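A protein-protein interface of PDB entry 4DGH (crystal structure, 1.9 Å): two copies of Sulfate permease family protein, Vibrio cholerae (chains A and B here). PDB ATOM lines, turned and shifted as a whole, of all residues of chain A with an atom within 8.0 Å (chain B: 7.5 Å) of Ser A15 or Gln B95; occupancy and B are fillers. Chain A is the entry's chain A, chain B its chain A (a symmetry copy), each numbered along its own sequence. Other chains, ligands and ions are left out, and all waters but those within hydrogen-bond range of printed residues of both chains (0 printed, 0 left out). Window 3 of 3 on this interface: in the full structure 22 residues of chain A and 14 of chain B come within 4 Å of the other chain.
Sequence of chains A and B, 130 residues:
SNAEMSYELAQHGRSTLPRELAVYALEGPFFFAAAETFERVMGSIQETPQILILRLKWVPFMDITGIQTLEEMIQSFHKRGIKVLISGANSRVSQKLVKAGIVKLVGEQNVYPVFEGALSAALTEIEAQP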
ATOM      1  N   MET A   5      -2.360  -3.744   1.900  1.00  0.00           N
ATOM      2  CA  MET A   5      -1.441  -3.682   3.046  1.00  0.00           C
ATOM      3  C   MET A   5      -2.243  -3.553   4.320  1.00  0.00           C
ATOM      4  O   MET A   5      -2.056  -4.375   5.246  1.00  0.00           O
ATOM      5  CB  MET A   5      -0.351  -2.589   2.905  1.00  0.00           C
ATOM      6  CG  MET A   5       0.964  -2.904   3.583  1.00  0.00           C
ATOM      7  SD  MET A   5       1.871  -1.184   3.322  1.00  0.00           S
ATOM      8  CE  MET A   5       2.744  -1.855   1.703  1.00  0.00           C
ATOM      9  N   SER A   6      -3.200  -2.621   4.386  1.00  0.00           N
ATOM     10  CA  SER A   6      -3.939  -2.464   5.639  1.00  0.00           C
ATOM     11  C   SER A   6      -4.726  -3.747   6.046  1.00  0.00           C
ATOM     12  O   SER A   6      -4.805  -4.085   7.213  1.00  0.00           O
ATOM     13  CB  SER A   6      -4.815  -1.187   5.647  1.00  0.00           C
ATOM     14  OG  SER A   6      -6.012  -1.427   4.938  1.00  0.00           O
ATOM     15  N   GLU A   8      -3.995  -7.081   5.385  1.00  0.00           N
ATOM     16  CA  GLU A   8      -3.067  -8.106   5.917  1.00  0.00           C
ATOM     17  C   GLU A   8      -2.430  -7.692   7.235  1.00  0.00           C
ATOM     18  O   GLU A   8      -2.271  -8.530   8.145  1.00  0.00           O
ATOM     19  CB  GLU A   8      -1.944  -8.418   4.950  1.00  0.00           C
ATOM     20  CG  GLU A   8      -2.288  -9.415   3.925  1.00  0.00           C
ATOM     21  CD  GLU A   8      -2.864 -10.713   4.501  1.00  0.00           C
ATOM     22  OE1 GLU A   8      -2.329 -11.287   5.475  1.00  0.00           O
ATOM     23  OE2 GLU A   8      -3.887 -11.136   3.950  1.00  0.00           O
ATOM     24  N   LEU A   9      -2.104  -6.417   7.345  1.00  0.00           N
ATOM     25  CA  LEU A   9      -1.615  -5.896   8.641  1.00  0.00           C
ATOM     26  C   LEU A   9      -2.624  -6.162   9.760  1.00  0.00           C
ATOM     27  O   LEU A   9      -2.254  -6.739  10.828  1.00  0.00           O
ATOM     28  CB  LEU A   9      -1.212  -4.435   8.561  1.00  0.00           C
ATOM     29  CG  LEU A   9       0.100  -4.131   7.745  1.00  0.00           C
ATOM     30  CD1 LEU A   9       0.299  -2.608   7.571  1.00  0.00           C
ATOM     31  CD2 LEU A   9       1.370  -4.702   8.397  1.00  0.00           C
ATOM     32  N   ALA A  10      -3.904  -5.836   9.510  1.00  0.00           N
ATOM     33  CA  ALA A  10      -4.908  -6.057  10.584  1.00  0.00           C
ATOM     34  C   ALA A  10      -5.075  -7.563  10.864  1.00  0.00           C
ATOM     35  O   ALA A  10      -5.243  -7.959  12.033  1.00  0.00           O
ATOM     36  CB  ALA A  10      -6.242  -5.408  10.230  1.00  0.00           C
ATOM     37  N   GLN A  11      -4.998  -8.414   9.841  1.00  0.00           N
ATOM     38  CA  GLN A  11      -5.038  -9.839  10.058  1.00  0.00           C
ATOM     39  C   GLN A  11      -3.954 -10.305  10.986  1.00  0.00           C
ATOM     40  O   GLN A  11      -4.163 -11.306  11.740  1.00  0.00           O
ATOM     41  CB  GLN A  11      -5.008 -10.608   8.756  1.00  0.00           C
ATOM     42  CG  GLN A  11      -6.272 -10.473   7.898  1.00  0.00           C
ATOM     43  CD  GLN A  11      -7.531 -11.040   8.573  1.00  0.00           C
ATOM     44  OE1 GLN A  11      -8.463 -10.280   8.968  1.00  0.00           O
ATOM     45  NE2 GLN A  11      -7.570 -12.364   8.727  1.00  0.00           N
ATOM     46  N   HIS A  12      -2.818  -9.604  10.979  1.00  0.00           N
ATOM     47  CA  HIS A  12      -1.744  -9.900  11.907  1.00  0.00           C
ATOM     48  C   HIS A  12      -1.690  -9.021  13.117  1.00  0.00           C
ATOM     49  O   HIS A  12      -0.647  -8.990  13.812  1.00  0.00           O
ATOM     50  CB  HIS A  12      -0.381  -9.881  11.169  1.00  0.00           C
ATOM     51  CG  HIS A  12      -0.236 -10.999  10.167  1.00  0.00           C
ATOM     52  ND1 HIS A  12       0.476 -12.110  10.416  1.00  0.00           N
ATOM     53  CD2 HIS A  12      -0.771 -11.152   8.881  1.00  0.00           C
ATOM     54  CE1 HIS A  12       0.393 -12.951   9.337  1.00  0.00           C
ATOM     55  NE2 HIS A  12      -0.369 -12.358   8.409  1.00  0.00           N
ATOM     56  N   GLY A  13      -2.787  -8.315  13.396  1.00  0.00           N
ATOM     57  CA  GLY A  13      -2.905  -7.464  14.565  1.00  0.00           C
ATOM     58  C   GLY A  13      -2.008  -6.223  14.588  1.00  0.00           C
ATOM     59  O   GLY A  13      -1.637  -5.735  15.685  1.00  0.00           O
ATOM     60  N   ARG A  14      -1.664  -5.697  13.409  1.00  0.00           N
ATOM     61  CA  ARG A  14      -0.806  -4.496  13.294  1.00  0.00           C
ATOM     62  C   ARG A  14      -1.520  -3.390  12.524  1.00  0.00           C
ATOM     63  O   ARG A  14      -2.450  -3.660  11.767  1.00  0.00           O
ATOM     64  CB  ARG A  14       0.471  -4.828  12.493  1.00  0.00           C
ATOM     65  CG  ARG A  14       1.263  -6.034  12.985  1.00  0.00           C
ATOM     66  CD  ARG A  14       2.635  -5.899  12.351  1.00  0.00           C
ATOM     67  NE  ARG A  14       3.106  -4.516  12.502  1.00  0.00           N
ATOM     68  CZ  ARG A  14       3.999  -4.138  13.394  1.00  0.00           C
ATOM     69  NH1 ARG A  14       4.375  -2.875  13.468  1.00  0.00           N
ATOM     70  NH2 ARG A  14       4.517  -5.039  14.227  1.00  0.00           N
ATOM     71  N   SER A  15      -1.071  -2.153  12.716  1.00  0.00           N
ATOM     72  CA  SER A  15      -1.557  -1.021  11.919  1.00  0.00           C
ATOM     73  C   SER A  15      -0.453  -0.496  10.980  1.00  0.00           C
ATOM     74  O   SER A  15      -0.748   0.140   9.959  1.00  0.00           O
ATOM     75  CB  SER A  15      -2.025   0.132  12.852  1.00  0.00           C
ATOM     76  OG  SER A  15      -1.178   0.172  14.002  1.00  0.00           O
ATOM     77  N   THR A  16       0.800  -0.781  11.335  1.00  0.00           N
ATOM     78  CA  THR A  16       1.947  -0.239  10.634  1.00  0.00           C
ATOM     79  C   THR A  16       2.857  -1.423  10.222  1.00  0.00           C
ATOM     80  O   THR A  16       2.887  -2.486  10.884  1.00  0.00           O
ATOM     81  CB  THR A  16       2.763   0.760  11.474  1.00  0.00           C
ATOM     82  OG1 THR A  16       3.429   0.088  12.538  1.00  0.00           O
ATOM     83  CG2 THR A  16       1.934   1.968  11.981  1.00  0.00           C
ATOM     84  N   LEU A  17       3.578  -1.218   9.118  1.00  0.00           N
ATOM     85  CA  LEU A  17       4.491  -2.217   8.616  1.00  0.00           C
ATOM     86  C   LEU A  17       5.551  -2.385   9.710  1.00  0.00           C
ATOM     87  O   LEU A  17       6.054  -1.379  10.283  1.00  0.00           O
ATOM     88  CB  LEU A  17       5.204  -1.641   7.389  1.00  0.00           C
ATOM     89  CG  LEU A  17       4.682  -1.926   5.980  1.00  0.00           C
ATOM     90  CD1 LEU A  17       5.698  -1.217   5.054  1.00  0.00           C
ATOM     91  CD2 LEU A  17       4.659  -3.432   5.703  1.00  0.00           C
ATOM     92  N   PRO A  18       5.846  -3.622  10.072  1.00  0.00           N
ATOM     93  CA  PRO A  18       6.905  -3.746  11.110  1.00  0.00           C
ATOM     94  C   PRO A  18       8.253  -3.354  10.600  1.00  0.00           C
ATOM     95  O   PRO A  18       8.522  -3.385   9.376  1.00  0.00           O
ATOM     96  CB  PRO A  18       6.887  -5.202  11.495  1.00  0.00           C
ATOM     97  CG  PRO A  18       6.394  -5.888  10.236  1.00  0.00           C
ATOM     98  CD  PRO A  18       5.463  -4.927   9.522  1.00  0.00           C
ATOM     99  N   ALA B  89       0.574  13.689   7.457  1.00  0.00           N
ATOM    100  CA  ALA B  89       0.827  12.217   7.569  1.00  0.00           C
ATOM    101  C   ALA B  89      -0.520  11.499   7.712  1.00  0.00           C
ATOM    102  O   ALA B  89      -1.333  11.945   8.517  1.00  0.00           O
ATOM    103  CB  ALA B  89       1.722  11.860   8.762  1.00  0.00           C
ATOM    104  N   ASN B  90      -0.783  10.429   6.971  1.00  0.00           N
ATOM    105  CA  ASN B  90      -2.028   9.674   7.251  1.00  0.00           C
ATOM    106  C   ASN B  90      -1.993   9.013   8.627  1.00  0.00           C
ATOM    107  O   ASN B  90      -1.004   9.118   9.310  1.00  0.00           O
ATOM    108  CB  ASN B  90      -2.374   8.682   6.188  1.00  0.00           C
ATOM    109  CG  ASN B  90      -1.355   7.550   6.066  1.00  0.00           C
ATOM    110  OD1 ASN B  90      -0.887   6.973   7.054  1.00  0.00           O
ATOM    111  ND2 ASN B  90      -1.135   7.142   4.825  1.00  0.00           N
ATOM    112  N   SER B  91      -3.068   8.313   9.007  1.00  0.00           N
ATOM    113  CA  SER B  91      -3.135   7.747  10.363  1.00  0.00           C
ATOM    114  C   SER B  91      -2.039   6.739  10.633  1.00  0.00           C
ATOM    115  O   SER B  91      -1.523   6.700  11.723  1.00  0.00           O
ATOM    116  CB  SER B  91      -4.537   7.162  10.701  1.00  0.00           C
ATOM    117  OG  SER B  91      -4.852   6.026   9.876  1.00  0.00           O
ATOM    118  N   ARG B  92      -1.661   5.921   9.670  1.00  0.00           N
ATOM    119  CA  ARG B  92      -0.617   4.999   9.940  1.00  0.00           C
ATOM    120  C   ARG B  92       0.793   5.568   9.898  1.00  0.00           C
ATOM    121  O   ARG B  92       1.630   5.255  10.727  1.00  0.00           O
ATOM    122  CB  ARG B  92      -0.767   3.710   9.131  1.00  0.00           C
ATOM    123  CG  ARG B  92      -0.150   3.712   7.784  1.00  0.00           C
ATOM    124  CD  ARG B  92      -0.355   2.313   7.181  1.00  0.00           C
ATOM    125  NE  ARG B  92      -0.375   2.443   5.744  1.00  0.00           N
ATOM    126  CZ  ARG B  92      -1.077   1.675   4.909  1.00  0.00           C
ATOM    127  NH1 ARG B  92      -1.848   0.668   5.363  1.00  0.00           N
ATOM    128  NH2 ARG B  92      -1.005   1.908   3.594  1.00  0.00           N
ATOM    129  N   VAL B  93       1.106   6.357   8.879  1.00  0.00           N
ATOM    130  CA  VAL B  93       2.393   7.030   8.883  1.00  0.00           C
ATOM    131  C   VAL B  93       2.536   7.908  10.150  1.00  0.00           C
ATOM    132  O   VAL B  93       3.657   8.016  10.666  1.00  0.00           O
ATOM    133  CB  VAL B  93       2.532   7.896   7.629  1.00  0.00           C
ATOM    134  CG1 VAL B  93       3.835   8.687   7.618  1.00  0.00           C
ATOM    135  CG2 VAL B  93       2.485   6.943   6.389  1.00  0.00           C
ATOM    136  N   SER B  94       1.450   8.541  10.579  1.00  0.00           N
ATOM    137  CA  SER B  94       1.474   9.375  11.840  1.00  0.00           C
ATOM    138  C   SER B  94       2.006   8.523  13.041  1.00  0.00           C
ATOM    139  O   SER B  94       2.860   8.963  13.768  1.00  0.00           O
ATOM    140  CB  SER B  94       0.080   9.902  12.190  1.00  0.00           C
ATOM    141  OG  SER B  94      -0.264  10.980  11.346  1.00  0.00           O
ATOM    142  N   GLN B  95       1.470   7.334  13.226  1.00  0.00           N
ATOM    143  CA  GLN B  95       1.987   6.393  14.297  1.00  0.00           C
ATOM    144  C   GLN B  95       3.435   6.028  14.060  1.00  0.00           C
ATOM    145  O   GLN B  95       4.190   5.970  15.012  1.00  0.00           O
ATOM    146  CB  GLN B  95       1.179   5.079  14.436  1.00  0.00           C
ATOM    147  CG  GLN B  95      -0.341   5.287  14.412  1.00  0.00           C
ATOM    148  CD  GLN B  95      -1.180   3.987  14.254  1.00  0.00           C
ATOM    149  OE1 GLN B  95      -2.008   3.848  13.320  1.00  0.00           O
ATOM    150  NE2 GLN B  95      -1.007   3.069  15.186  1.00  0.00           N
ATOM    151  N   LYS B  96       3.808   5.757  12.799  1.00  0.00           N
ATOM    152  CA  LYS B  96       5.200   5.393  12.492  1.00  0.00           C
ATOM    153  C   LYS B  96       6.156   6.537  12.823  1.00  0.00           C
ATOM    154  O   LYS B  96       7.244   6.310  13.320  1.00  0.00           O
ATOM    155  CB  LYS B  96       5.394   5.076  11.003  1.00  0.00           C
ATOM    156  CG  LYS B  96       5.631   3.683  10.636  1.00  0.00           C
ATOM    157  CD  LYS B  96       7.087   3.364  10.581  1.00  0.00           C
ATOM    158  CE  LYS B  96       7.078   1.881  10.725  1.00  0.00           C
ATOM    159  NZ  LYS B  96       6.820   1.278   9.414  1.00  0.00           N
ATOM    160  N   LEU B  97       5.768   7.781  12.503  1.00  0.00           N
ATOM    161  CA  LEU B  97       6.620   8.927  12.753  1.00  0.00           C
ATOM    162  C   LEU B  97       6.953   9.049  14.303  1.00  0.00           C
ATOM    163  O   LEU B  97       8.066   9.433  14.675  1.00  0.00           O
ATOM    164  CB  LEU B  97       5.931  10.210  12.292  1.00  0.00           C
ATOM    165  CG  LEU B  97       5.747  10.319  10.712  1.00  0.00           C
ATOM    166  CD1 LEU B  97       5.224  11.715  10.422  1.00  0.00           C
ATOM    167  CD2 LEU B  97       7.062  10.080   9.997  1.00  0.00           C
ATOM    168  N   VAL B  98       5.960   8.740  15.133  1.00  0.00           N
ATOM    169  CA  VAL B  98       6.138   8.773  16.603  1.00  0.00           C
ATOM    170  C   VAL B  98       7.082   7.615  16.992  1.00  0.00           C
ATOM    171  O   VAL B  98       8.175   7.846  17.519  1.00  0.00           O
ATOM    172  CB  VAL B  98       4.795   8.628  17.337  1.00  0.00           C
ATOM    173  CG1 VAL B  98       5.017   8.432  18.875  1.00  0.00           C
ATOM    174  CG2 VAL B  98       3.934   9.870  17.085  1.00  0.00           C
ATOM    175  N   LYS B  99       6.727   6.405  16.601  1.00  0.00           N
ATOM    176  CA  LYS B  99       7.521   5.239  17.003  1.00  0.00           C
ATOM    177  C   LYS B  99       8.973   5.301  16.532  1.00  0.00           C
ATOM    178  O   LYS B  99       9.853   4.817  17.231  1.00  0.00           O
ATOM    179  CB  LYS B  99       6.902   3.914  16.499  1.00  0.00           C
ATOM    180  CG  LYS B  99       5.390   3.723  16.759  1.00  0.00           C
ATOM    181  CD  LYS B  99       4.940   2.246  16.633  1.00  0.00           C
ATOM    182  CE  LYS B  99       5.564   1.494  15.420  1.00  0.00           C
ATOM    183  NZ  LYS B  99       4.877   1.681  14.097  1.00  0.00           N
ATOM    184  N   ALA B 100       9.222   5.886  15.355  1.00  0.00           N
ATOM    185  CA  ALA B 100      10.553   5.977  14.808  1.00  0.00           C
ATOM    186  C   ALA B 100      11.402   7.108  15.317  1.00  0.00           C
ATOM    187  O   ALA B 100      12.606   7.130  15.026  1.00  0.00           O
ATOM    188  CB  ALA B 100      10.487   6.039  13.293  1.00  0.00           C
ATOM    189  N   GLY B 101      10.836   8.012  16.119  1.00  0.00           N
ATOM    190  CA  GLY B 101      11.592   9.160  16.597  1.00  0.00           C
ATOM    191  C   GLY B 101      11.607  10.381  15.659  1.00  0.00           C
ATOM    192  O   GLY B 101      12.384  11.333  15.874  1.00  0.00           O
ATOM    193  N   VAL B 103       9.050  12.401  15.238  1.00  0.00           N
ATOM    194  CA  VAL B 103       8.310  13.471  15.945  1.00  0.00           C
ATOM    195  C   VAL B 103       9.252  14.108  16.966  1.00  0.00           C
ATOM    196  O   VAL B 103       9.311  15.320  17.049  1.00  0.00           O
ATOM    197  CB  VAL B 103       7.005  12.952  16.583  1.00  0.00           C
ATOM    198  CG1 VAL B 103       6.410  13.979  17.558  1.00  0.00           C
ATOM    199  CG2 VAL B 103       6.009  12.567  15.494  1.00  0.00           C
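NH1 of Arg B92 touches CB of Ser A6, 3.5 Å away.
Ser A15 touches Arg B92 (O to CD, 3.5 Å).
Thr A16 touches Arg B92.
No position is printed for both chains.
Of the 13 printed residues of chain A, 4 touch a printed residue of chain B.
Hydrophobic or aromatic side chains of chain A within 4 Å of the printed part of chain B: Leu A17.
Of the 14 printed residues of chain B, 4 touch a printed residue of chain A.
Among the printed residues, no Asp or Glu carboxylate lies within 4 Å of a Lys or Arg side-chain nitrogen of the other chain.
The backbone NH (N) of Arg B92 sits at hydrogen-bond distance from the side-chain amide oxygen (OD1) of Asn B90.
The backbone carbonyl oxygen of Ser B91 lies close to the side-chain amide oxygen of Gln B95 (3.3 Å).
O of Thr A16 sits at hydrogen-bond distance from NE of Arg A14 (2.6 Å).
The side-chain hydroxyl (OG) of Ser A15 lies within hydrogen-bond range of the side-chain amide nitrogen (NE2) of Gln B95.
The side-chain hydroxyl of Thr A16 lies within hydrogen-bond range of the side-chain amino group of Lys B99 (2.7 Å).
The backbone carbonyl oxygen (O) of Leu A17 is in hydrogen-bond range of the side-chain amino group (NZ) of Lys B96 (2.9 Å).
Of the printed residues of chain B, Ser A6 touches Arg B92 (3.5 Å).
His A12 touches none of the printed residues of chain B.
Ser A15 touches just these residues of chain B: Arg B92 and Gln B95.
Of the printed residues of chain B, Thr A16 touches Arg B92 and Lys B99.
Printed residues of chain B within 4 Å of Leu A17: Lys B96.
Asn B90 touches none of the printed residues of chain A.
Printed residues of chain A within 4 Å of Arg B92: Ser A6, Ser A15 and Thr A16.
Of the printed residues of chain A, Lys B99 touches Thr A16 (2.7 Å).
The nearest residue of chain B that does not touch Ser A15 is Lys B99 (6.2 Å).
The nearest residue of chain A that does not touch Gln B95 is Thr A16 (4.03 Å).
The nearest printed residue of chain B that does not touch Ser A6 is Ser B91 (8.4 Å).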
